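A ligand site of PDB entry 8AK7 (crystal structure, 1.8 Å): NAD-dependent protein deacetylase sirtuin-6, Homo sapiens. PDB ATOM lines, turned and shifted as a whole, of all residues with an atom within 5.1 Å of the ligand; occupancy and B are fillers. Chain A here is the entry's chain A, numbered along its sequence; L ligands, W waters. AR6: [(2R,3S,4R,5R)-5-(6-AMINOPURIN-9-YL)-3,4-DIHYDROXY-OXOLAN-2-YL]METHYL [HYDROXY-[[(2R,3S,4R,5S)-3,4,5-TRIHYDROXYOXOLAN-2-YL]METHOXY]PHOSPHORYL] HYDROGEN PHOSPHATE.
A ring nitrogen (ND1) of His 127 sits at hydrogen-bond distance from an oxygen (O3D) of the ligand (2.6 Å).
An oxygen (O3') of the ligand lies within hydrogen-bond range of the side-chain amide nitrogen of Asn 234, at 2.6 Å.
O2B of the ligand sits at hydrogen-bond distance from N of Ser 210.
OG of Ser 210 lies within hydrogen-bond range of O1A of the ligand.
The side-chain hydroxyl (OG1) of Thr 209 sits at hydrogen-bond distance from an oxygen (O2B) of the ligand (2.8 Å).
O2' of the ligand sits close to N of Gln 236 (3.4 Å).
The side-chain amide oxygen (OE1) of Gln 236 is in hydrogen-bond range of an oxygen (O3') of the ligand (2.8 Å).
An oxygen (O2A) of the ligand lies within hydrogen-bond range of the backbone NH (N) of Arg 59 (2.8 Å).
An oxygen (O1A) of the ligand is in salt-bridge range of the guanidinium group (NH1) of Arg 59 (2.8 Å).
A nitrogen (N7) of the ligand sits at hydrogen-bond distance from the side-chain hydroxyl (OG1) of Thr 51 (2.8 Å).
N of Val 252 lies within hydrogen-bond range of N1 of the ligand (2.9 Å).
The backbone NH of Ala 47 lies within hydrogen-bond range of an oxygen (O1B) of the ligand, at 2.9 Å.
The backbone carbonyl oxygen (O) of Gln 107 is in hydrogen-bond range of an oxygen (O3D) of the ligand (2.9 Å).
The backbone NH (N) of Phe 58 lies within hydrogen-bond range of an oxygen (O2A) of the ligand, 2.9 Å away.
O1D of the ligand lies within hydrogen-bond range of NE1 of Trp 65 (3.3 Å).
The backbone NH (N) of Leu 235 sits at hydrogen-bond distance from a nitrogen (N3) of the ligand (3.3 Å).
N7 of the ligand lies close to O of Gly 48 (3.3 Å).
O of Gly 208 sits close to O4' of the ligand (3.3 Å).
Gly 46 touches the ligand (CA to O1B, 3.1 Å).
OD2 of Asp 57 touches C8 of the ligand, at 3.1 Å.
CH2 of Trp 182 touches O1D of the ligand, 3.9 Å away.
CG1 of Ile 213 touches O4D of the ligand, at 3.5 Å.
Gly 250 touches the ligand (O to C2, 3.4 Å).
Tyr 251 touches the ligand.
Hydrophobic or aromatic side chains that line the ligand: Ala 47, Phe 58, Trp 65, His 127, Trp 182, Ile 213, Leu 235, Tyr 251 and Val 252.
Of the 28 residues printed, 21 come within 4 Å of the ligand.
The nearest printed residue that does not touch the ligand is Gly 60 (4.04 Å).
The side-chain amide nitrogen (ND2) of Asn 234 lies within hydrogen-bond range of the backbone carbonyl oxygen (O) of Gln 236, at 2.9 Å.
NE2 of Gln 212 lies within hydrogen-bond range of OG of Ser 210, 3.1 Å away.
OG1 of Thr 209 is in hydrogen-bond range of N of Leu 211.
The side-chain amide nitrogen (NE2) of Gln 236 is in hydrogen-bond range of the backbone carbonyl oxygen (O) of Arg 59 (3.1 Å).
The side-chain hydroxyl of Thr 51 sits at hydrogen-bond distance from the backbone carbonyl oxygen of Gly 48, 3.2 Å away.
O of Gly 208 lies within hydrogen-bond range of N of Ala 47 (3.1 Å).
N of Gly 60 is in hydrogen-bond range of OD1 of Asp 57, at 2.9 Å.
O of Val 233 is in hydrogen-bond range of N of Gly 208 (3.0 Å).
Water W2 lies within hydrogen-bond range of an oxygen (O1B) of the ligand, the side-chain amide oxygen (OD1) of Asn 108 and the backbone carbonyl oxygen (O) of Gln 107.
Water W1 lies within hydrogen-bond range of N6 of the ligand (3.1 Å) and N of Val 252 (3.5 Å).
Water W4 lies within hydrogen-bond range of O of Gly 48 (2.9 Å), OG1 of Thr 51 (3.2 Å) and N6 of the ligand (3.4 Å).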
ATOM      1  N   GLU A  16     -24.388  32.708   6.005  1.00  0.00           N
ATOM      2  CA  GLU A  16     -23.178  32.680   6.867  1.00  0.00           C
ATOM      3  C   GLU A  16     -22.299  33.869   6.483  1.00  0.00           C
ATOM      4  O   GLU A  16     -22.388  34.314   5.335  1.00  0.00           O
ATOM      5  CB  GLU A  16     -22.527  31.298   6.739  1.00  0.00           C
ATOM      6  CG  GLU A  16     -23.378  30.205   7.347  1.00  0.00           C
ATOM      7  CD  GLU A  16     -22.684  28.869   7.432  1.00  0.00           C
ATOM      8  OE1 GLU A  16     -21.869  28.586   6.533  1.00  0.00           O
ATOM      9  OE2 GLU A  16     -22.934  28.119   8.402  1.00  0.00           O
ATOM     10  N   GLY A  46     -24.599  27.778  22.571  1.00  0.00           N
ATOM     11  CA  GLY A  46     -25.736  27.169  21.859  1.00  0.00           C
ATOM     12  C   GLY A  46     -25.193  26.155  20.858  1.00  0.00           C
ATOM     13  O   GLY A  46     -23.971  25.870  20.926  1.00  0.00           O
ATOM     14  N   ALA A  47     -26.022  25.729  19.930  1.00  0.00           N
ATOM     15  CA  ALA A  47     -25.900  24.452  19.184  1.00  0.00           C
ATOM     16  C   ALA A  47     -24.724  24.507  18.204  1.00  0.00           C
ATOM     17  O   ALA A  47     -24.179  23.397  17.903  1.00  0.00           O
ATOM     18  CB  ALA A  47     -27.199  24.119  18.465  1.00  0.00           C
ATOM     19  N   GLY A  48     -24.319  25.713  17.810  1.00  0.00           N
ATOM     20  CA  GLY A  48     -23.135  25.995  16.983  1.00  0.00           C
ATOM     21  C   GLY A  48     -21.863  25.395  17.549  1.00  0.00           C
ATOM     22  O   GLY A  48     -20.997  24.996  16.764  1.00  0.00           O
ATOM     23  N   THR A  51     -21.764  21.411  16.299  1.00  0.00           N
ATOM     24  CA  THR A  51     -21.882  21.068  14.858  1.00  0.00           C
ATOM     25  C   THR A  51     -20.620  20.306  14.410  1.00  0.00           C
ATOM     26  O   THR A  51     -20.783  19.383  13.600  1.00  0.00           O
ATOM     27  CB  THR A  51     -22.166  22.261  13.932  1.00  0.00           C
ATOM     28  OG1 THR A  51     -21.203  23.314  14.081  1.00  0.00           O
ATOM     29  CG2 THR A  51     -23.593  22.785  14.061  1.00  0.00           C
ATOM     30  N   ASP A  57     -27.190  21.971  14.261  1.00  0.00           N
ATOM     31  CA  ASP A  57     -27.828  23.106  14.985  1.00  0.00           C
ATOM     32  C   ASP A  57     -29.296  23.209  14.544  1.00  0.00           C
ATOM     33  O   ASP A  57     -29.789  22.294  13.849  1.00  0.00           O
ATOM     34  CB  ASP A  57     -27.010  24.387  14.835  1.00  0.00           C
ATOM     35  CG  ASP A  57     -26.943  25.004  13.435  1.00  0.00           C
ATOM     36  OD1 ASP A  57     -27.781  24.640  12.557  1.00  0.00           O
ATOM     37  OD2 ASP A  57     -26.059  25.852  13.224  1.00  0.00           O
ATOM     38  N   PHE A  58     -29.988  24.263  14.998  1.00  0.00           N
ATOM     39  CA  PHE A  58     -31.436  24.484  14.791  1.00  0.00           C
ATOM     40  C   PHE A  58     -31.673  25.415  13.592  1.00  0.00           C
ATOM     41  O   PHE A  58     -32.541  25.107  12.768  1.00  0.00           O
ATOM     42  CB  PHE A  58     -32.064  25.019  16.085  1.00  0.00           C
ATOM     43  CG  PHE A  58     -32.089  24.002  17.202  1.00  0.00           C
ATOM     44  CD1 PHE A  58     -33.095  23.044  17.253  1.00  0.00           C
ATOM     45  CD2 PHE A  58     -31.106  23.982  18.186  1.00  0.00           C
ATOM     46  CE1 PHE A  58     -33.114  22.089  18.249  1.00  0.00           C
ATOM     47  CE2 PHE A  58     -31.122  23.020  19.188  1.00  0.00           C
ATOM     48  CZ  PHE A  58     -32.144  22.086  19.226  1.00  0.00           C
ATOM     49  N   ARG A  59     -30.920  26.518  13.483  1.00  0.00           N
ATOM     50  CA  ARG A  59     -31.231  27.653  12.589  1.00  0.00           C
ATOM     51  C   ARG A  59     -30.096  27.900  11.592  1.00  0.00           C
ATOM     52  O   ARG A  59     -30.229  28.814  10.779  1.00  0.00           O
ATOM     53  CB  ARG A  59     -31.603  28.903  13.391  1.00  0.00           C
ATOM     54  CG  ARG A  59     -32.798  28.647  14.292  1.00  0.00           C
ATOM     55  CD  ARG A  59     -33.225  29.873  15.084  1.00  0.00           C
ATOM     56  NE  ARG A  59     -34.285  29.461  15.976  1.00  0.00           N
ATOM     57  CZ  ARG A  59     -34.132  28.816  17.135  1.00  0.00           C
ATOM     58  NH1 ARG A  59     -32.935  28.536  17.618  1.00  0.00           N
ATOM     59  NH2 ARG A  59     -35.194  28.480  17.835  1.00  0.00           N
ATOM     60  N   GLY A  60     -29.076  27.047  11.546  1.00  0.00           N
ATOM     61  CA  GLY A  60     -27.985  27.153  10.539  1.00  0.00           C
ATOM     62  C   GLY A  60     -28.452  26.716   9.141  1.00  0.00           C
ATOM     63  O   GLY A  60     -29.582  26.286   8.963  1.00  0.00           O
ATOM     64  N   TRP A  65     -34.620  23.190  12.330  1.00  0.00           N
ATOM     65  CA  TRP A  65     -35.761  24.033  11.884  1.00  0.00           C
ATOM     66  C   TRP A  65     -35.582  24.487  10.435  1.00  0.00           C
ATOM     67  O   TRP A  65     -36.590  24.455   9.678  1.00  0.00           O
ATOM     68  CB  TRP A  65     -35.986  25.243  12.795  1.00  0.00           C
ATOM     69  CG  TRP A  65     -36.092  24.988  14.265  1.00  0.00           C
ATOM     70  CD1 TRP A  65     -35.731  25.874  15.233  1.00  0.00           C
ATOM     71  CD2 TRP A  65     -36.633  23.839  14.943  1.00  0.00           C
ATOM     72  NE1 TRP A  65     -35.989  25.354  16.469  1.00  0.00           N
ATOM     73  CE2 TRP A  65     -36.562  24.111  16.326  1.00  0.00           C
ATOM     74  CE3 TRP A  65     -37.203  22.624  14.530  1.00  0.00           C
ATOM     75  CZ2 TRP A  65     -36.983  23.202  17.288  1.00  0.00           C
ATOM     76  CZ3 TRP A  65     -37.619  21.727  15.488  1.00  0.00           C
ATOM     77  CH2 TRP A  65     -37.512  22.009  16.848  1.00  0.00           C
ATOM     78  N   GLN A 107     -27.649  26.658  26.241  1.00  0.00           N
ATOM     79  CA  GLN A 107     -29.000  26.287  25.762  1.00  0.00           C
ATOM     80  C   GLN A 107     -28.979  24.836  25.253  1.00  0.00           C
ATOM     81  O   GLN A 107     -30.045  24.344  24.897  1.00  0.00           O
ATOM     82  CB  GLN A 107     -29.407  27.325  24.720  1.00  0.00           C
ATOM     83  CG  GLN A 107     -29.499  28.738  25.272  1.00  0.00           C
ATOM     84  CD  GLN A 107     -29.650  29.734  24.151  1.00  0.00           C
ATOM     85  OE1 GLN A 107     -30.685  29.795  23.481  1.00  0.00           O
ATOM     86  NE2 GLN A 107     -28.591  30.487  23.893  1.00  0.00           N
ATOM     87  N   ASN A 108     -27.819  24.172  25.243  1.00  0.00           N
ATOM     88  CA  ASN A 108     -27.646  22.852  24.592  1.00  0.00           C
ATOM     89  C   ASN A 108     -28.169  21.764  25.539  1.00  0.00           C
ATOM     90  O   ASN A 108     -27.917  21.849  26.770  1.00  0.00           O
ATOM     91  CB  ASN A 108     -26.202  22.591  24.175  1.00  0.00           C
ATOM     92  CG  ASN A 108     -25.728  23.597  23.160  1.00  0.00           C
ATOM     93  OD1 ASN A 108     -26.534  24.302  22.561  1.00  0.00           O
ATOM     94  ND2 ASN A 108     -24.420  23.682  22.949  1.00  0.00           N
ATOM     95  N   HIS A 127     -32.019  24.627  29.051  1.00  0.00           N
ATOM     96  CA  HIS A 127     -33.018  23.884  28.246  1.00  0.00           C
ATOM     97  C   HIS A 127     -33.057  22.399  28.660  1.00  0.00           C
ATOM     98  O   HIS A 127     -33.874  21.649  28.095  1.00  0.00           O
ATOM     99  CB  HIS A 127     -32.743  24.128  26.754  1.00  0.00           C
ATOM    100  CG  HIS A 127     -32.854  25.569  26.357  1.00  0.00           C
ATOM    101  ND1 HIS A 127     -32.521  26.058  25.070  1.00  0.00           N
ATOM    102  CD2 HIS A 127     -33.316  26.634  27.059  1.00  0.00           C
ATOM    103  CE1 HIS A 127     -32.757  27.339  25.024  1.00  0.00           C
ATOM    104  NE2 HIS A 127     -33.272  27.722  26.235  1.00  0.00           N
ATOM    105  N   TRP A 182     -41.862  23.515  24.475  1.00  0.00           N
ATOM    106  CA  TRP A 182     -42.062  24.948  24.102  1.00  0.00           C
ATOM    107  C   TRP A 182     -42.736  25.721  25.249  1.00  0.00           C
ATOM    108  O   TRP A 182     -42.336  26.880  25.473  1.00  0.00           O
ATOM    109  CB  TRP A 182     -42.869  25.069  22.802  1.00  0.00           C
ATOM    110  CG  TRP A 182     -42.100  24.623  21.595  1.00  0.00           C
ATOM    111  CD1 TRP A 182     -42.168  23.401  20.982  1.00  0.00           C
ATOM    112  CD2 TRP A 182     -41.099  25.369  20.890  1.00  0.00           C
ATOM    113  NE1 TRP A 182     -41.291  23.349  19.934  1.00  0.00           N
ATOM    114  CE2 TRP A 182     -40.620  24.549  19.855  1.00  0.00           C
ATOM    115  CE3 TRP A 182     -40.581  26.668  21.026  1.00  0.00           C
ATOM    116  CZ2 TRP A 182     -39.650  24.979  18.954  1.00  0.00           C
ATOM    117  CZ3 TRP A 182     -39.609  27.090  20.146  1.00  0.00           C
ATOM    118  CH2 TRP A 182     -39.156  26.250  19.120  1.00  0.00           C
ATOM    119  N   GLY A 208     -21.577  30.210  19.073  1.00  0.00           N
ATOM    120  CA  GLY A 208     -22.492  29.372  18.282  1.00  0.00           C
ATOM    121  C   GLY A 208     -23.924  29.371  18.796  1.00  0.00           C
ATOM    122  O   GLY A 208     -24.491  28.280  18.896  1.00  0.00           O
ATOM    123  N   THR A 209     -24.469  30.542  19.170  1.00  0.00           N
ATOM    124  CA  THR A 209     -25.897  30.783  19.471  1.00  0.00           C
ATOM    125  C   THR A 209     -26.401  32.016  18.693  1.00  0.00           C
ATOM    126  O   THR A 209     -25.731  33.042  18.699  1.00  0.00           O
ATOM    127  CB  THR A 209     -26.159  30.989  20.959  1.00  0.00           C
ATOM    128  OG1 THR A 209     -27.572  31.220  21.067  1.00  0.00           O
ATOM    129  CG2 THR A 209     -25.375  32.116  21.576  1.00  0.00           C
ATOM    130  N   SER A 210     -27.597  31.949  18.087  1.00  0.00           N
ATOM    131  CA  SER A 210     -28.190  33.076  17.327  1.00  0.00           C
ATOM    132  C   SER A 210     -28.974  34.020  18.265  1.00  0.00           C
ATOM    133  O   SER A 210     -29.460  35.017  17.754  1.00  0.00           O
ATOM    134  CB  SER A 210     -29.048  32.606  16.166  1.00  0.00           C
ATOM    135  OG  SER A 210     -30.146  31.827  16.567  1.00  0.00           O
ATOM    136  N   LEU A 211     -29.123  33.646  19.542  1.00  0.00           N
ATOM    137  CA  LEU A 211     -29.635  34.537  20.646  1.00  0.00           C
ATOM    138  C   LEU A 211     -31.114  34.894  20.452  1.00  0.00           C
ATOM    139  O   LEU A 211     -31.555  35.946  20.997  1.00  0.00           O
ATOM    140  CB  LEU A 211     -28.728  35.764  20.738  1.00  0.00           C
ATOM    141  CG  LEU A 211     -27.247  35.460  21.025  1.00  0.00           C
ATOM    142  CD1 LEU A 211     -26.376  36.692  20.862  1.00  0.00           C
ATOM    143  CD2 LEU A 211     -27.065  34.840  22.415  1.00  0.00           C
ATOM    144  N   GLN A 212     -31.881  34.025  19.792  1.00  0.00           N
ATOM    145  CA  GLN A 212     -33.274  34.294  19.353  1.00  0.00           C
ATOM    146  C   GLN A 212     -34.293  33.830  20.409  1.00  0.00           C
ATOM    147  O   GLN A 212     -35.469  34.189  20.285  1.00  0.00           O
ATOM    148  CB  GLN A 212     -33.542  33.616  18.008  1.00  0.00           C
ATOM    149  CG  GLN A 212     -32.815  34.258  16.842  1.00  0.00           C
ATOM    150  CD  GLN A 212     -33.281  33.622  15.547  1.00  0.00           C
ATOM    151  OE1 GLN A 212     -34.458  33.662  15.223  1.00  0.00           O
ATOM    152  NE2 GLN A 212     -32.358  33.080  14.773  1.00  0.00           N
ATOM    153  N   ILE A 213     -33.875  33.054  21.414  1.00  0.00           N
ATOM    154  CA  ILE A 213     -34.784  32.488  22.450  1.00  0.00           C
ATOM    155  C   ILE A 213     -34.653  33.312  23.725  1.00  0.00           C
ATOM    156  O   ILE A 213     -33.511  33.492  24.188  1.00  0.00           O
ATOM    157  CB  ILE A 213     -34.513  30.989  22.681  1.00  0.00           C
ATOM    158  CG1 ILE A 213     -34.757  30.175  21.414  1.00  0.00           C
ATOM    159  CG2 ILE A 213     -35.351  30.475  23.847  1.00  0.00           C
ATOM    160  CD1 ILE A 213     -36.215  29.942  21.103  1.00  0.00           C
ATOM    161  N   VAL A 233     -19.528  35.321  19.007  1.00  0.00           N
ATOM    162  CA  VAL A 233     -18.852  34.476  17.981  1.00  0.00           C
ATOM    163  C   VAL A 233     -19.933  33.622  17.288  1.00  0.00           C
ATOM    164  O   VAL A 233     -20.615  32.820  17.971  1.00  0.00           O
ATOM    165  CB  VAL A 233     -17.712  33.645  18.615  1.00  0.00           C
ATOM    166  CG1 VAL A 233     -16.953  32.829  17.575  1.00  0.00           C
ATOM    167  CG2 VAL A 233     -16.749  34.502  19.415  1.00  0.00           C
ATOM    168  N   ASN A 234     -20.082  33.763  15.970  1.00  0.00           N
ATOM    169  CA  ASN A 234     -21.171  33.084  15.227  1.00  0.00           C
ATOM    170  C   ASN A 234     -21.001  33.237  13.716  1.00  0.00           C
ATOM    171  O   ASN A 234     -20.637  34.341  13.231  1.00  0.00           O
ATOM    172  CB  ASN A 234     -22.547  33.651  15.606  1.00  0.00           C
ATOM    173  CG  ASN A 234     -23.624  32.595  15.571  1.00  0.00           C
ATOM    174  OD1 ASN A 234     -23.568  31.633  16.317  1.00  0.00           O
ATOM    175  ND2 ASN A 234     -24.665  32.824  14.800  1.00  0.00           N
ATOM    176  N   LEU A 235     -21.310  32.180  12.984  1.00  0.00           N
ATOM    177  CA  LEU A 235     -21.239  32.183  11.513  1.00  0.00           C
ATOM    178  C   LEU A 235     -22.353  33.069  10.918  1.00  0.00           C
ATOM    179  O   LEU A 235     -22.072  33.780   9.940  1.00  0.00           O
ATOM    180  CB  LEU A 235     -21.282  30.744  11.019  1.00  0.00           C
ATOM    181  CG  LEU A 235     -19.975  29.975  11.172  1.00  0.00           C
ATOM    182  CD1 LEU A 235     -20.200  28.516  10.810  1.00  0.00           C
ATOM    183  CD2 LEU A 235     -18.874  30.587  10.319  1.00  0.00           C
ATOM    184  N   GLN A 236     -23.541  33.059  11.521  1.00  0.00           N
ATOM    185  CA  GLN A 236     -24.749  33.805  11.075  1.00  0.00           C
ATOM    186  C   GLN A 236     -24.911  35.047  11.941  1.00  0.00           C
ATOM    187  O   GLN A 236     -24.356  35.112  13.044  1.00  0.00           O
ATOM    188  CB  GLN A 236     -26.024  32.983  11.274  1.00  0.00           C
ATOM    189  CG  GLN A 236     -26.193  31.862  10.265  1.00  0.00           C
ATOM    190  CD  GLN A 236     -27.406  31.015  10.555  1.00  0.00           C
ATOM    191  OE1 GLN A 236     -27.840  30.862  11.714  1.00  0.00           O
ATOM    192  NE2 GLN A 236     -27.996  30.482   9.509  1.00  0.00           N
ATOM    193  N   PRO A 237     -25.682  36.037  11.463  1.00  0.00           N
ATOM    194  CA  PRO A 237     -26.181  37.124  12.307  1.00  0.00           C
ATOM    195  C   PRO A 237     -26.876  36.550  13.549  1.00  0.00           C
ATOM    196  O   PRO A 237     -27.320  35.441  13.512  1.00  0.00           O
ATOM    197  CB  PRO A 237     -27.195  37.871  11.412  1.00  0.00           C
ATOM    198  CG  PRO A 237     -26.716  37.563   9.998  1.00  0.00           C
ATOM    199  CD  PRO A 237     -26.124  36.166  10.061  1.00  0.00           C
ATOM    200  N   GLY A 250     -16.604  33.271  12.299  1.00  0.00           N
ATOM    201  CA  GLY A 250     -15.734  32.128  11.979  1.00  0.00           C
ATOM    202  C   GLY A 250     -16.177  30.892  12.746  1.00  0.00           C
ATOM    203  O   GLY A 250     -17.040  31.038  13.642  1.00  0.00           O
ATOM    204  N   TYR A 251     -15.627  29.742  12.390  1.00  0.00           N
ATOM    205  CA  TYR A 251     -15.837  28.456  13.094  1.00  0.00           C
ATOM    206  C   TYR A 251     -15.348  28.622  14.533  1.00  0.00           C
ATOM    207  O   TYR A 251     -14.214  29.090  14.730  1.00  0.00           O
ATOM    208  CB  TYR A 251     -15.145  27.328  12.336  1.00  0.00           C
ATOM    209  CG  TYR A 251     -15.736  27.108  10.970  1.00  0.00           C
ATOM    210  CD1 TYR A 251     -16.944  26.456  10.811  1.00  0.00           C
ATOM    211  CD2 TYR A 251     -15.102  27.597   9.823  1.00  0.00           C
ATOM    212  CE1 TYR A 251     -17.506  26.263   9.561  1.00  0.00           C
ATOM    213  CE2 TYR A 251     -15.648  27.399   8.574  1.00  0.00           C
ATOM    214  CZ  TYR A 251     -16.854  26.739   8.436  1.00  0.00           C
ATOM    215  OH  TYR A 251     -17.393  26.565   7.191  1.00  0.00           O
ATOM    216  N   VAL A 252     -16.220  28.330  15.487  1.00  0.00           N
ATOM    217  CA  VAL A 252     -15.931  28.555  16.921  1.00  0.00           C
ATOM    218  C   VAL A 252     -14.669  27.745  17.293  1.00  0.00           C
ATOM    219  O   VAL A 252     -13.853  28.274  18.045  1.00  0.00           O
ATOM    220  CB  VAL A 252     -17.150  28.297  17.818  1.00  0.00           C
ATOM    221  CG1 VAL A 252     -17.597  26.826  17.835  1.00  0.00           C
ATOM    222  CG2 VAL A 252     -16.908  28.810  19.211  1.00  0.00           C
HETATM  223  N1  AR6 L   1     -18.890  27.984  14.461  1.00  0.00           N
HETATM  224  C2  AR6 L   1     -19.599  29.103  14.662  1.00  0.00           C
HETATM  225  N3  AR6 L   1     -20.924  29.272  14.594  1.00  0.00           N
HETATM  226  C4  AR6 L   1     -21.560  28.128  14.282  1.00  0.00           C
HETATM  227  C5  AR6 L   1     -20.953  26.913  14.012  1.00  0.00           C
HETATM  228  C6  AR6 L   1     -19.553  26.855  14.104  1.00  0.00           C
HETATM  229  N6  AR6 L   1     -18.837  25.742  13.905  1.00  0.00           N
HETATM  230  N7  AR6 L   1     -21.944  25.976  13.708  1.00  0.00           N
HETATM  231  C8  AR6 L   1     -23.087  26.615  13.833  1.00  0.00           C
HETATM  232  N9  AR6 L   1     -22.910  27.939  14.136  1.00  0.00           N
HETATM  233  PA  AR6 L   1     -29.249  28.157  16.592  1.00  0.00           P
HETATM  234  PB  AR6 L   1     -29.315  28.030  19.559  1.00  0.00           P
HETATM  235  C1' AR6 L   1     -23.921  28.956  14.377  1.00  0.00           C
HETATM  236  O1A AR6 L   1     -30.352  29.170  16.627  1.00  0.00           O
HETATM  237  O1B AR6 L   1     -28.491  27.169  20.485  1.00  0.00           O
HETATM  238  C1D AR6 L   1     -33.969  25.796  19.852  1.00  0.00           C
HETATM  239  O1D AR6 L   1     -35.338  25.683  19.641  1.00  0.00           O
HETATM  240  C2' AR6 L   1     -25.119  29.058  13.433  1.00  0.00           C
HETATM  241  O2' AR6 L   1     -24.786  29.998  12.469  1.00  0.00           O
HETATM  242  O2A AR6 L   1     -29.175  27.038  15.580  1.00  0.00           O
HETATM  243  O2B AR6 L   1     -29.078  29.490  19.535  1.00  0.00           O
HETATM  244  C2D AR6 L   1     -33.498  25.002  21.077  1.00  0.00           C
HETATM  245  O2D AR6 L   1     -34.443  24.991  22.130  1.00  0.00           O
HETATM  246  C3' AR6 L   1     -26.242  29.603  14.339  1.00  0.00           C
HETATM  247  O3' AR6 L   1     -26.434  30.984  14.104  1.00  0.00           O
HETATM  248  O3A AR6 L   1     -29.156  27.466  18.047  1.00  0.00           O
HETATM  249  C3D AR6 L   1     -32.201  25.746  21.426  1.00  0.00           C
HETATM  250  O3D AR6 L   1     -31.670  25.499  22.730  1.00  0.00           O
HETATM  251  C4' AR6 L   1     -25.761  29.305  15.752  1.00  0.00           C
HETATM  252  O4' AR6 L   1     -24.467  28.668  15.627  1.00  0.00           O
HETATM  253  C4D AR6 L   1     -32.657  27.189  21.235  1.00  0.00           C
HETATM  254  O4D AR6 L   1     -33.625  27.152  20.159  1.00  0.00           O
HETATM  255  C5' AR6 L   1     -26.629  28.365  16.529  1.00  0.00           C
HETATM  256  O5' AR6 L   1     -27.931  28.964  16.534  1.00  0.00           O
HETATM  257  C5D AR6 L   1     -31.586  28.188  20.881  1.00  0.00           C
HETATM  258  O5D AR6 L   1     -30.855  27.693  19.721  1.00  0.00           O
HETATM  259  O   HOH W   1     -16.256  24.843  15.261  1.00  0.00           O
HETATM  260  O   HOH W   2     -29.175  24.827  21.716  1.00  0.00           O
HETATM  261  O   HOH W   3     -31.281  31.148  19.003  1.00  0.00           O
HETATM  262  O   HOH W   4     -18.838  23.215  16.188  1.00  0.00           O
HETATM  263  O   HOH W   5     -24.663  25.755  10.873  1.00  0.00           O
